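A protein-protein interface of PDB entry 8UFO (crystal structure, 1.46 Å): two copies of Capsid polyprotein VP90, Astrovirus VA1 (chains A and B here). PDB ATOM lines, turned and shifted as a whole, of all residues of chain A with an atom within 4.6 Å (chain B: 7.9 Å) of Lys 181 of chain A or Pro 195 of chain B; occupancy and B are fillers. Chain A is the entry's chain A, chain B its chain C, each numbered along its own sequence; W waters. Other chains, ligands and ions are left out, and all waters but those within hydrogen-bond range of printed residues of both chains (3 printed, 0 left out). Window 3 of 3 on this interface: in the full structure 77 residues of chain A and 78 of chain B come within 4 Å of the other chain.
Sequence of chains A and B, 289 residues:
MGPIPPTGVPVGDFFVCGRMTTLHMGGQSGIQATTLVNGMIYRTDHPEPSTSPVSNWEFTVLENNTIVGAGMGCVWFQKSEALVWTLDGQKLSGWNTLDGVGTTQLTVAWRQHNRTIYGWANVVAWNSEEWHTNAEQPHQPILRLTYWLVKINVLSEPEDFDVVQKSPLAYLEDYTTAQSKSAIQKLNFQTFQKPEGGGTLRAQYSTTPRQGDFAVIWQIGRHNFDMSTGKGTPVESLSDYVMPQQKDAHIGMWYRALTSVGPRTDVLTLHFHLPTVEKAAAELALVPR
OE1 of Gln 190 of chain B sits at hydrogen-bond distance from OG of Ser 180 of chain A (2.6 Å). The backbone carbonyl oxygen of Thr 191 of chain B is in hydrogen-bond range of the backbone NH of Ser 180 of chain A, 3.1 Å away. The side-chain hydroxyl (OH) of Tyr 175 of chain B lies within hydrogen-bond range of the backbone carbonyl oxygen (O) of Leu 172 of chain A (2.6 Å). The backbone carbonyl oxygen (O) of Ser 180 of chain A lies within hydrogen-bond range of the backbone NH (N) of Gln 193 of chain B, at 2.9 Å. The backbone carbonyl oxygen of Gln 193 of chain B is in hydrogen-bond range of the backbone NH of Ser 182 of chain A. The backbone carbonyl oxygen of Pro 195 of chain B lies within hydrogen-bond range of the side-chain amino group of Lys 181 of chain A (3.0 Å).
The side-chain amide oxygen of Gln 193 of chain B is in hydrogen-bond range of the backbone NH of Gly 198 of chain B, at 3.4 Å. The side-chain carboxylate (OE2) of Glu 196 of chain B is in salt-bridge range of the side-chain amino group (NZ) of Lys 194 of chain B (3.1 Å). The backbone carbonyl oxygen (O) of Tyr 171 of chain A is in hydrogen-bond range of the backbone NH (N) of Ala 183 of chain A. The backbone carbonyl oxygen of Glu 173 of chain A lies within hydrogen-bond range of the backbone NH of Lys 181 of chain A (2.8 Å). The backbone NH (N) of Gly 26 of chain B is in hydrogen-bond range of the backbone carbonyl oxygen (O) of Leu 36 of chain B (3.0 Å). N of Gly 199 of chain B sits at hydrogen-bond distance from OE1 of Gln 193 of chain B.
Tyr 171 of chain A touches Thr 177 of chain B (CZ to CG2, 3.8 Å). Gln 190 of chain B touches Leu 172 of chain A. O of Gln 193 of chain B touches CA of Lys 181 of chain A, at 3.3 Å. Lys 181 of chain A touches Lys 194 of chain B. Ser 182 of chain A touches Pro 195 of chain B (O to CD, 3.7 Å). Leu 36 of chain B touches Ala 183 of chain A. Ile 184 of chain A touches Gly 26 of chain B. Ile 31 of chain B touches Ile 184 of chain A. CD of Pro 195 of chain B touches CG1 of Ile 184 of chain A, 3.7 Å away. CD1 of Leu 201 of chain B touches CD1 of Ile 184 of chain A, 3.8 Å away.
Of chain B, only Gln 193 (3.3 Å), Lys 194 (3.9 Å) and Pro 195 (3.0 Å) come within 4 Å of Lys 181 of chain A. Ser 180 of chain A touches four residues of chain B. Of the printed residues of chain A, Leu 201 of chain B touches Ile 184. Printed residues of chain A within 4 Å of Phe 192 of chain B: Leu 172 (3.8 Å), Ser 180 (3.7 Å) and Ser 182 (3.3 Å). Of the printed residues of chain A, Gln 193 of chain B touches Ser 180, Lys 181 and Ser 182. Gly 199 of chain B touches none of the printed residues of chain A. Thr 200 of chain B touches none of the printed residues of chain A. The nearest residue of chain B that does not touch Lys 181 of chain A is Gly 197 of chain B (4.1 Å). The nearest residue of chain A that does not touch Pro 195 of chain B is Ala 183 of chain A (4.4 Å). The nearest printed residue of chain B that does not touch Ser 182 of chain A is Leu 201 of chain B (4.04 Å).
Printed residues of chain B that touch a printed residue of chain A: Gly 26, Gly 27, Ile 31, Leu 36, Tyr 175, Thr 177, Gln 190, Thr 191, Phe 192, Gln 193, Lys 194, Pro 195 and Leu 201. Hydrophobic or aromatic side chains of chain B that line the printed part of chain A: Ile 31, Leu 36, Tyr 175, Phe 192, Pro 195 and Leu 201. Along chain B the printed residues that touch a printed residue of chain A span positions 26 to 201. Hydrophobic or aromatic side chains of chain A that line the printed part of chain B: Tyr 171, Leu 172 and Ile 184. Among the printed residues, 22 pairs touch across the chains. Among the printed residues, no Asp or Glu carboxylate lies within 4 Å of a Lys or Arg side-chain nitrogen of the other chain.
No position is printed for both chains. Of the 22 pairs that touch across the chains among the printed residues, none has its exchanged pair printed and touching as well.
Water W2 lies within hydrogen-bond range of the backbone carbonyl oxygen (O) of Ile 184 of chain A (2.7 Å), the backbone carbonyl oxygen (O) of Gly 26 of chain B (2.7 Å) and the backbone NH (N) of Leu 36 of chain B (2.8 Å). Water W3 bridges the side-chain hydroxyl of Tyr 175 of chain B (2.7 Å) and the backbone NH of Leu 172 of chain A (3.1 Å). Water W1 bridges O of Asp 174 of chain A (2.8 Å) and NE2 of Gln 193 of chain B (3.0 Å).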
ATOM      1  N   TYR A 171     -14.260  -4.548  15.367  1.00  0.00           N
ATOM      2  CA  TYR A 171     -13.375  -3.499  15.880  1.00  0.00           C
ATOM      3  C   TYR A 171     -12.122  -3.469  15.010  1.00  0.00           C
ATOM      4  O   TYR A 171     -11.283  -4.372  15.087  1.00  0.00           O
ATOM      5  CB  TYR A 171     -13.035  -3.752  17.344  1.00  0.00           C
ATOM      6  CG  TYR A 171     -12.365  -2.581  18.025  1.00  0.00           C
ATOM      7  CD1 TYR A 171     -10.984  -2.431  17.996  1.00  0.00           C
ATOM      8  CD2 TYR A 171     -13.120  -1.622  18.685  1.00  0.00           C
ATOM      9  CE1 TYR A 171     -10.366  -1.364  18.631  1.00  0.00           C
ATOM     10  CE2 TYR A 171     -12.513  -0.544  19.325  1.00  0.00           C
ATOM     11  CZ  TYR A 171     -11.140  -0.427  19.287  1.00  0.00           C
ATOM     12  OH  TYR A 171     -10.534   0.642  19.919  1.00  0.00           O
ATOM     13  N   LEU A 172     -12.014  -2.455  14.155  1.00  0.00           N
ATOM     14  CA  LEU A 172     -10.987  -2.411  13.124  1.00  0.00           C
ATOM     15  C   LEU A 172      -9.995  -1.295  13.417  1.00  0.00           C
ATOM     16  O   LEU A 172     -10.389  -0.159  13.697  1.00  0.00           O
ATOM     17  CB  LEU A 172     -11.598  -2.206  11.736  1.00  0.00           C
ATOM     18  CG  LEU A 172     -12.677  -3.240  11.357  1.00  0.00           C
ATOM     19  CD1 LEU A 172     -13.273  -2.891   9.986  1.00  0.00           C
ATOM     20  CD2 LEU A 172     -12.170  -4.682  11.398  1.00  0.00           C
ATOM     21  N   GLU A 173      -8.716  -1.635  13.357  1.00  0.00           N
ATOM     22  CA  GLU A 173      -7.633  -0.675  13.526  1.00  0.00           C
ATOM     23  C   GLU A 173      -6.752  -0.712  12.291  1.00  0.00           C
ATOM     24  O   GLU A 173      -6.841  -1.622  11.459  1.00  0.00           O
ATOM     25  CB  GLU A 173      -6.823  -1.001  14.781  1.00  0.00           C
ATOM     26  CG  GLU A 173      -7.650  -0.878  16.058  1.00  0.00           C
ATOM     27  CD  GLU A 173      -6.856  -1.197  17.303  1.00  0.00           C
ATOM     28  OE1 GLU A 173      -6.378  -2.342  17.433  1.00  0.00           O
ATOM     29  OE2 GLU A 173      -6.710  -0.299  18.156  1.00  0.00           O
ATOM     30  N   ASP A 174      -5.891   0.299  12.160  1.00  0.00           N
ATOM     31  CA  ASP A 174      -5.020   0.418  10.991  1.00  0.00           C
ATOM     32  C   ASP A 174      -5.830   0.238   9.710  1.00  0.00           C
ATOM     33  O   ASP A 174      -5.488  -0.542   8.817  1.00  0.00           O
ATOM     34  CB  ASP A 174      -3.851  -0.566  11.062  1.00  0.00           C
ATOM     35  CG  ASP A 174      -2.883  -0.244  12.182  1.00  0.00           C
ATOM     36  OD1 ASP A 174      -2.990   0.857  12.760  1.00  0.00           O
ATOM     37  OD2 ASP A 174      -2.005  -1.084  12.464  1.00  0.00           O
ATOM     38  N   SER A 180      -7.760  -4.180   7.124  1.00  0.00           N
ATOM     39  CA  SER A 180      -7.634  -3.630   8.466  1.00  0.00           C
ATOM     40  C   SER A 180      -7.191  -4.737   9.407  1.00  0.00           C
ATOM     41  O   SER A 180      -7.226  -5.923   9.068  1.00  0.00           O
ATOM     42  CB  SER A 180      -8.953  -3.022   8.953  1.00  0.00           C
ATOM     43  OG  SER A 180      -9.907  -4.047   9.110  1.00  0.00           O
ATOM     44  N   LYS A 181      -6.757  -4.330  10.595  1.00  0.00           N
ATOM     45  CA  LYS A 181      -6.475  -5.249  11.688  1.00  0.00           C
ATOM     46  C   LYS A 181      -7.756  -5.402  12.503  1.00  0.00           C
ATOM     47  O   LYS A 181      -8.214  -4.454  13.152  1.00  0.00           O
ATOM     48  CB  LYS A 181      -5.334  -4.721  12.553  1.00  0.00           C
ATOM     49  CG  LYS A 181      -3.972  -4.869  11.897  1.00  0.00           C
ATOM     50  CD  LYS A 181      -2.885  -4.228  12.733  1.00  0.00           C
ATOM     51  CE  LYS A 181      -1.541  -4.391  12.043  1.00  0.00           C
ATOM     52  NZ  LYS A 181      -0.428  -4.501  13.028  1.00  0.00           N
ATOM     53  N   SER A 182      -8.329  -6.600  12.460  1.00  0.00           N
ATOM     54  CA  SER A 182      -9.601  -6.915  13.101  1.00  0.00           C
ATOM     55  C   SER A 182      -9.336  -7.529  14.469  1.00  0.00           C
ATOM     56  O   SER A 182      -8.697  -8.584  14.566  1.00  0.00           O
ATOM     57  CB  SER A 182     -10.359  -7.913  12.227  1.00  0.00           C
ATOM     58  OG  SER A 182      -9.536  -9.027  11.891  1.00  0.00           O
ATOM     59  N   ALA A 183      -9.841  -6.884  15.519  1.00  0.00           N
ATOM     60  CA  ALA A 183      -9.668  -7.420  16.864  1.00  0.00           C
ATOM     61  C   ALA A 183     -10.345  -8.784  16.983  1.00  0.00           C
ATOM     62  O   ALA A 183     -11.470  -8.985  16.514  1.00  0.00           O
ATOM     63  CB  ALA A 183     -10.252  -6.442  17.882  1.00  0.00           C
ATOM     64  N   ILE A 184      -9.645  -9.725  17.624  1.00  0.00           N
ATOM     65  CA  ILE A 184     -10.022 -11.140  17.612  1.00  0.00           C
ATOM     66  C   ILE A 184     -11.250 -11.417  18.472  1.00  0.00           C
ATOM     67  O   ILE A 184     -12.014 -12.354  18.195  1.00  0.00           O
ATOM     68  CB  ILE A 184      -8.808 -12.000  18.050  1.00  0.00           C
ATOM     69  CG1 ILE A 184      -7.607 -11.763  17.121  1.00  0.00           C
ATOM     70  CG2 ILE A 184      -9.169 -13.483  18.102  1.00  0.00           C
ATOM     71  CD1 ILE A 184      -7.945 -11.945  15.631  1.00  0.00           C
ATOM     72  N   GLY B  26     -12.068 -16.477  13.130  1.00  0.00           N
ATOM     73  CA  GLY B  26     -10.851 -15.776  12.753  1.00  0.00           C
ATOM     74  C   GLY B  26     -10.002 -15.362  13.933  1.00  0.00           C
ATOM     75  O   GLY B  26     -10.436 -14.572  14.772  1.00  0.00           O
ATOM     76  N   GLY B  27      -8.764 -15.852  13.983  1.00  0.00           N
ATOM     77  CA  GLY B  27      -8.011 -15.709  15.212  1.00  0.00           C
ATOM     78  C   GLY B  27      -6.556 -15.312  15.072  1.00  0.00           C
ATOM     79  O   GLY B  27      -6.114 -14.826  14.031  1.00  0.00           O
ATOM     80  N   GLN B  28      -5.821 -15.497  16.163  1.00  0.00           N
ATOM     81  CA  GLN B  28      -4.377 -15.332  16.210  1.00  0.00           C
ATOM     82  C   GLN B  28      -3.900 -16.345  17.232  1.00  0.00           C
ATOM     83  O   GLN B  28      -4.565 -16.544  18.251  1.00  0.00           O
ATOM     84  CB  GLN B  28      -4.050 -13.926  16.700  1.00  0.00           C
ATOM     85  CG  GLN B  28      -2.567 -13.636  16.890  1.00  0.00           C
ATOM     86  CD  GLN B  28      -2.318 -12.153  17.095  1.00  0.00           C
ATOM     87  OE1 GLN B  28      -2.584 -11.346  16.205  1.00  0.00           O
ATOM     88  NE2 GLN B  28      -1.832 -11.782  18.282  1.00  0.00           N
ATOM     89  N   ILE B  31      -4.964 -16.752  21.113  1.00  0.00           N
ATOM     90  CA  ILE B  31      -6.107 -15.914  21.474  1.00  0.00           C
ATOM     91  C   ILE B  31      -7.346 -16.634  20.953  1.00  0.00           C
ATOM     92  O   ILE B  31      -7.450 -16.906  19.750  1.00  0.00           O
ATOM     93  CB  ILE B  31      -6.023 -14.520  20.833  1.00  0.00           C
ATOM     94  CG1 ILE B  31      -4.772 -13.768  21.290  1.00  0.00           C
ATOM     95  CG2 ILE B  31      -7.247 -13.699  21.228  1.00  0.00           C
ATOM     96  CD1 ILE B  31      -4.647 -12.392  20.653  1.00  0.00           C
ATOM     97  N   LEU B  36     -15.057 -13.142  15.085  1.00  0.00           N
ATOM     98  CA  LEU B  36     -14.859 -12.960  13.642  1.00  0.00           C
ATOM     99  C   LEU B  36     -15.401 -14.186  12.927  1.00  0.00           C
ATOM    100  O   LEU B  36     -14.684 -15.149  12.640  1.00  0.00           O
ATOM    101  CB  LEU B  36     -13.393 -12.690  13.327  1.00  0.00           C
ATOM    102  CG  LEU B  36     -12.877 -11.415  14.011  1.00  0.00           C
ATOM    103  CD1 LEU B  36     -11.397 -11.269  13.680  1.00  0.00           C
ATOM    104  CD2 LEU B  36     -13.647 -10.159  13.572  1.00  0.00           C
ATOM    105  N   TYR B 175     -12.520   7.089   8.490  1.00  0.00           N
ATOM    106  CA  TYR B 175     -12.783   6.111   9.541  1.00  0.00           C
ATOM    107  C   TYR B 175     -11.954   6.363  10.795  1.00  0.00           C
ATOM    108  O   TYR B 175     -10.738   6.588  10.712  1.00  0.00           O
ATOM    109  CB  TYR B 175     -12.483   4.700   9.024  1.00  0.00           C
ATOM    110  CG  TYR B 175     -12.545   3.642  10.106  1.00  0.00           C
ATOM    111  CD1 TYR B 175     -11.436   3.355  10.904  1.00  0.00           C
ATOM    112  CD2 TYR B 175     -13.720   2.918  10.322  1.00  0.00           C
ATOM    113  CE1 TYR B 175     -11.499   2.407  11.901  1.00  0.00           C
ATOM    114  CE2 TYR B 175     -13.787   1.957  11.310  1.00  0.00           C
ATOM    115  CZ  TYR B 175     -12.680   1.702  12.087  1.00  0.00           C
ATOM    116  OH  TYR B 175     -12.743   0.758  13.079  1.00  0.00           O
ATOM    117  N   THR B 177     -12.315   4.404  15.036  1.00  0.00           N
ATOM    118  CA  THR B 177     -13.125   3.425  15.767  1.00  0.00           C
ATOM    119  C   THR B 177     -14.421   4.017  16.316  1.00  0.00           C
ATOM    120  O   THR B 177     -15.376   3.268  16.568  1.00  0.00           O
ATOM    121  CB  THR B 177     -12.319   2.769  16.888  1.00  0.00           C
ATOM    122  OG1 THR B 177     -11.849   3.779  17.787  1.00  0.00           O
ATOM    123  CG2 THR B 177     -11.140   1.987  16.312  1.00  0.00           C
ATOM    124  N   GLN B 190     -13.229  -6.978   2.566  1.00  0.00           N
ATOM    125  CA  GLN B 190     -11.834  -6.572   2.697  1.00  0.00           C
ATOM    126  C   GLN B 190     -11.052  -7.666   3.411  1.00  0.00           C
ATOM    127  O   GLN B 190     -11.616  -8.595   3.999  1.00  0.00           O
ATOM    128  CB  GLN B 190     -11.669  -5.225   3.431  1.00  0.00           C
ATOM    129  CG  GLN B 190     -11.808  -5.319   4.935  1.00  0.00           C
ATOM    130  CD  GLN B 190     -11.518  -4.024   5.698  1.00  0.00           C
ATOM    131  OE1 GLN B 190     -11.374  -4.046   6.921  1.00  0.00           O
ATOM    132  NE2 GLN B 190     -11.459  -2.896   4.993  1.00  0.00           N
ATOM    133  N   THR B 191      -9.731  -7.559   3.364  1.00  0.00           N
ATOM    134  CA  THR B 191      -8.906  -8.451   4.158  1.00  0.00           C
ATOM    135  C   THR B 191      -8.960  -8.040   5.626  1.00  0.00           C
ATOM    136  O   THR B 191      -8.734  -6.877   5.973  1.00  0.00           O
ATOM    137  CB  THR B 191      -7.472  -8.379   3.653  1.00  0.00           C
ATOM    138  OG1 THR B 191      -7.437  -8.809   2.293  1.00  0.00           O
ATOM    139  CG2 THR B 191      -6.575  -9.252   4.477  1.00  0.00           C
ATOM    140  N   PHE B 192      -9.286  -8.997   6.493  1.00  0.00           N
ATOM    141  CA  PHE B 192      -9.157  -8.818   7.935  1.00  0.00           C
ATOM    142  C   PHE B 192      -7.877  -9.546   8.324  1.00  0.00           C
ATOM    143  O   PHE B 192      -7.776 -10.763   8.137  1.00  0.00           O
ATOM    144  CB  PHE B 192     -10.329  -9.475   8.682  1.00  0.00           C
ATOM    145  CG  PHE B 192     -11.596  -8.622   8.810  1.00  0.00           C
ATOM    146  CD1 PHE B 192     -11.760  -7.406   8.152  1.00  0.00           C
ATOM    147  CD2 PHE B 192     -12.644  -9.100   9.602  1.00  0.00           C
ATOM    148  CE1 PHE B 192     -12.952  -6.683   8.287  1.00  0.00           C
ATOM    149  CE2 PHE B 192     -13.827  -8.378   9.760  1.00  0.00           C
ATOM    150  CZ  PHE B 192     -13.991  -7.181   9.095  1.00  0.00           C
ATOM    151  N   GLN B 193      -6.893  -8.811   8.835  1.00  0.00           N
ATOM    152  CA  GLN B 193      -5.667  -9.434   9.312  1.00  0.00           C
ATOM    153  C   GLN B 193      -5.619  -9.386  10.833  1.00  0.00           C
ATOM    154  O   GLN B 193      -6.223  -8.514  11.473  1.00  0.00           O
ATOM    155  CB  GLN B 193      -4.410  -8.771   8.716  1.00  0.00           C
ATOM    156  CG  GLN B 193      -4.133  -7.354   9.183  1.00  0.00           C
ATOM    157  CD  GLN B 193      -2.761  -6.866   8.761  1.00  0.00           C
ATOM    158  OE1 GLN B 193      -1.823  -7.655   8.645  1.00  0.00           O
ATOM    159  NE2 GLN B 193      -2.641  -5.561   8.540  1.00  0.00           N
ATOM    160  N   LYS B 194      -4.898 -10.347  11.408  1.00  0.00           N
ATOM    161  CA  LYS B 194      -4.755 -10.420  12.851  1.00  0.00           C
ATOM    162  C   LYS B 194      -3.968  -9.211  13.377  1.00  0.00           C
ATOM    163  O   LYS B 194      -3.166  -8.610  12.651  1.00  0.00           O
ATOM    164  CB  LYS B 194      -4.078 -11.730  13.277  1.00  0.00           C
ATOM    165  CG  LYS B 194      -2.775 -12.067  12.554  1.00  0.00           C
ATOM    166  CD  LYS B 194      -2.417 -13.542  12.781  1.00  0.00           C
ATOM    167  CE  LYS B 194      -1.267 -14.051  11.918  1.00  0.00           C
ATOM    168  NZ  LYS B 194      -0.110 -13.141  11.818  1.00  0.00           N
ATOM    169  N   PRO B 195      -4.201  -8.827  14.632  1.00  0.00           N
ATOM    170  CA  PRO B 195      -3.539  -7.627  15.179  1.00  0.00           C
ATOM    171  C   PRO B 195      -2.021  -7.653  15.095  1.00  0.00           C
ATOM    172  O   PRO B 195      -1.414  -6.586  14.943  1.00  0.00           O
ATOM    173  CB  PRO B 195      -4.028  -7.602  16.632  1.00  0.00           C
ATOM    174  CG  PRO B 195      -5.375  -8.264  16.569  1.00  0.00           C
ATOM    175  CD  PRO B 195      -5.250  -9.345  15.531  1.00  0.00           C
ATOM    176  N   GLU B 196      -1.384  -8.827  15.175  1.00  0.00           N
ATOM    177  CA  GLU B 196       0.073  -8.866  15.055  1.00  0.00           C
ATOM    178  C   GLU B 196       0.557  -8.668  13.623  1.00  0.00           C
ATOM    179  O   GLU B 196       1.771  -8.589  13.403  1.00  0.00           O
ATOM    180  CB  GLU B 196       0.623 -10.168  15.637  1.00  0.00           C
ATOM    181  CG  GLU B 196       0.314 -11.403  14.815  1.00  0.00           C
ATOM    182  CD  GLU B 196       1.013 -12.648  15.337  1.00  0.00           C
ATOM    183  OE1 GLU B 196       1.756 -12.539  16.334  1.00  0.00           O
ATOM    184  OE2 GLU B 196       0.818 -13.735  14.752  1.00  0.00           O
ATOM    185  N   GLY B 197      -0.344  -8.583  12.657  1.00  0.00           N
ATOM    186  CA  GLY B 197       0.048  -8.346  11.287  1.00  0.00           C
ATOM    187  C   GLY B 197       0.335  -9.626  10.530  1.00  0.00           C
ATOM    188  O   GLY B 197       0.002 -10.738  10.948  1.00  0.00           O
ATOM    189  N   GLY B 198       0.976  -9.451   9.373  1.00  0.00           N
ATOM    190  CA  GLY B 198       1.281 -10.550   8.483  1.00  0.00           C
ATOM    191  C   GLY B 198       0.354 -10.673   7.293  1.00  0.00           C
ATOM    192  O   GLY B 198       0.598 -11.521   6.417  1.00  0.00           O
ATOM    193  N   GLY B 199      -0.698  -9.854   7.231  1.00  0.00           N
ATOM    194  CA  GLY B 199      -1.660  -9.922   6.150  1.00  0.00           C
ATOM    195  C   GLY B 199      -2.628 -11.083   6.233  1.00  0.00           C
ATOM    196  O   GLY B 199      -3.469 -11.230   5.333  1.00  0.00           O
ATOM    197  N   THR B 200      -2.521 -11.909   7.264  1.00  0.00           N
ATOM    198  CA  THR B 200      -3.245 -13.159   7.399  1.00  0.00           C
ATOM    199  C   THR B 200      -4.036 -13.134   8.700  1.00  0.00           C
ATOM    200  O   THR B 200      -3.877 -12.252   9.546  1.00  0.00           O
ATOM    201  CB  THR B 200      -2.264 -14.341   7.414  1.00  0.00           C
ATOM    202  OG1 THR B 200      -1.328 -14.155   8.487  1.00  0.00           O
ATOM    203  CG2 THR B 200      -1.509 -14.438   6.091  1.00  0.00           C
ATOM    204  N   LEU B 201      -4.892 -14.135   8.846  1.00  0.00           N
ATOM    205  CA  LEU B 201      -5.741 -14.320  10.010  1.00  0.00           C
ATOM    206  C   LEU B 201      -5.779 -15.820  10.266  1.00  0.00           C
ATOM    207  O   LEU B 201      -5.761 -16.614   9.318  1.00  0.00           O
ATOM    208  CB  LEU B 201      -7.144 -13.786   9.684  1.00  0.00           C
ATOM    209  CG  LEU B 201      -8.198 -13.726  10.792  1.00  0.00           C
ATOM    210  CD1 LEU B 201      -7.827 -12.686  11.861  1.00  0.00           C
ATOM    211  CD2 LEU B 201      -9.553 -13.414  10.172  1.00  0.00           C
HETATM  212  O   HOH W   1      -4.026  -2.915   8.508  1.00  0.00           O
HETATM  213  O   HOH W   2     -12.662 -14.071  16.275  1.00  0.00           O
HETATM  214  O   HOH W   3     -14.548  -0.658  14.494  1.00  0.00           O
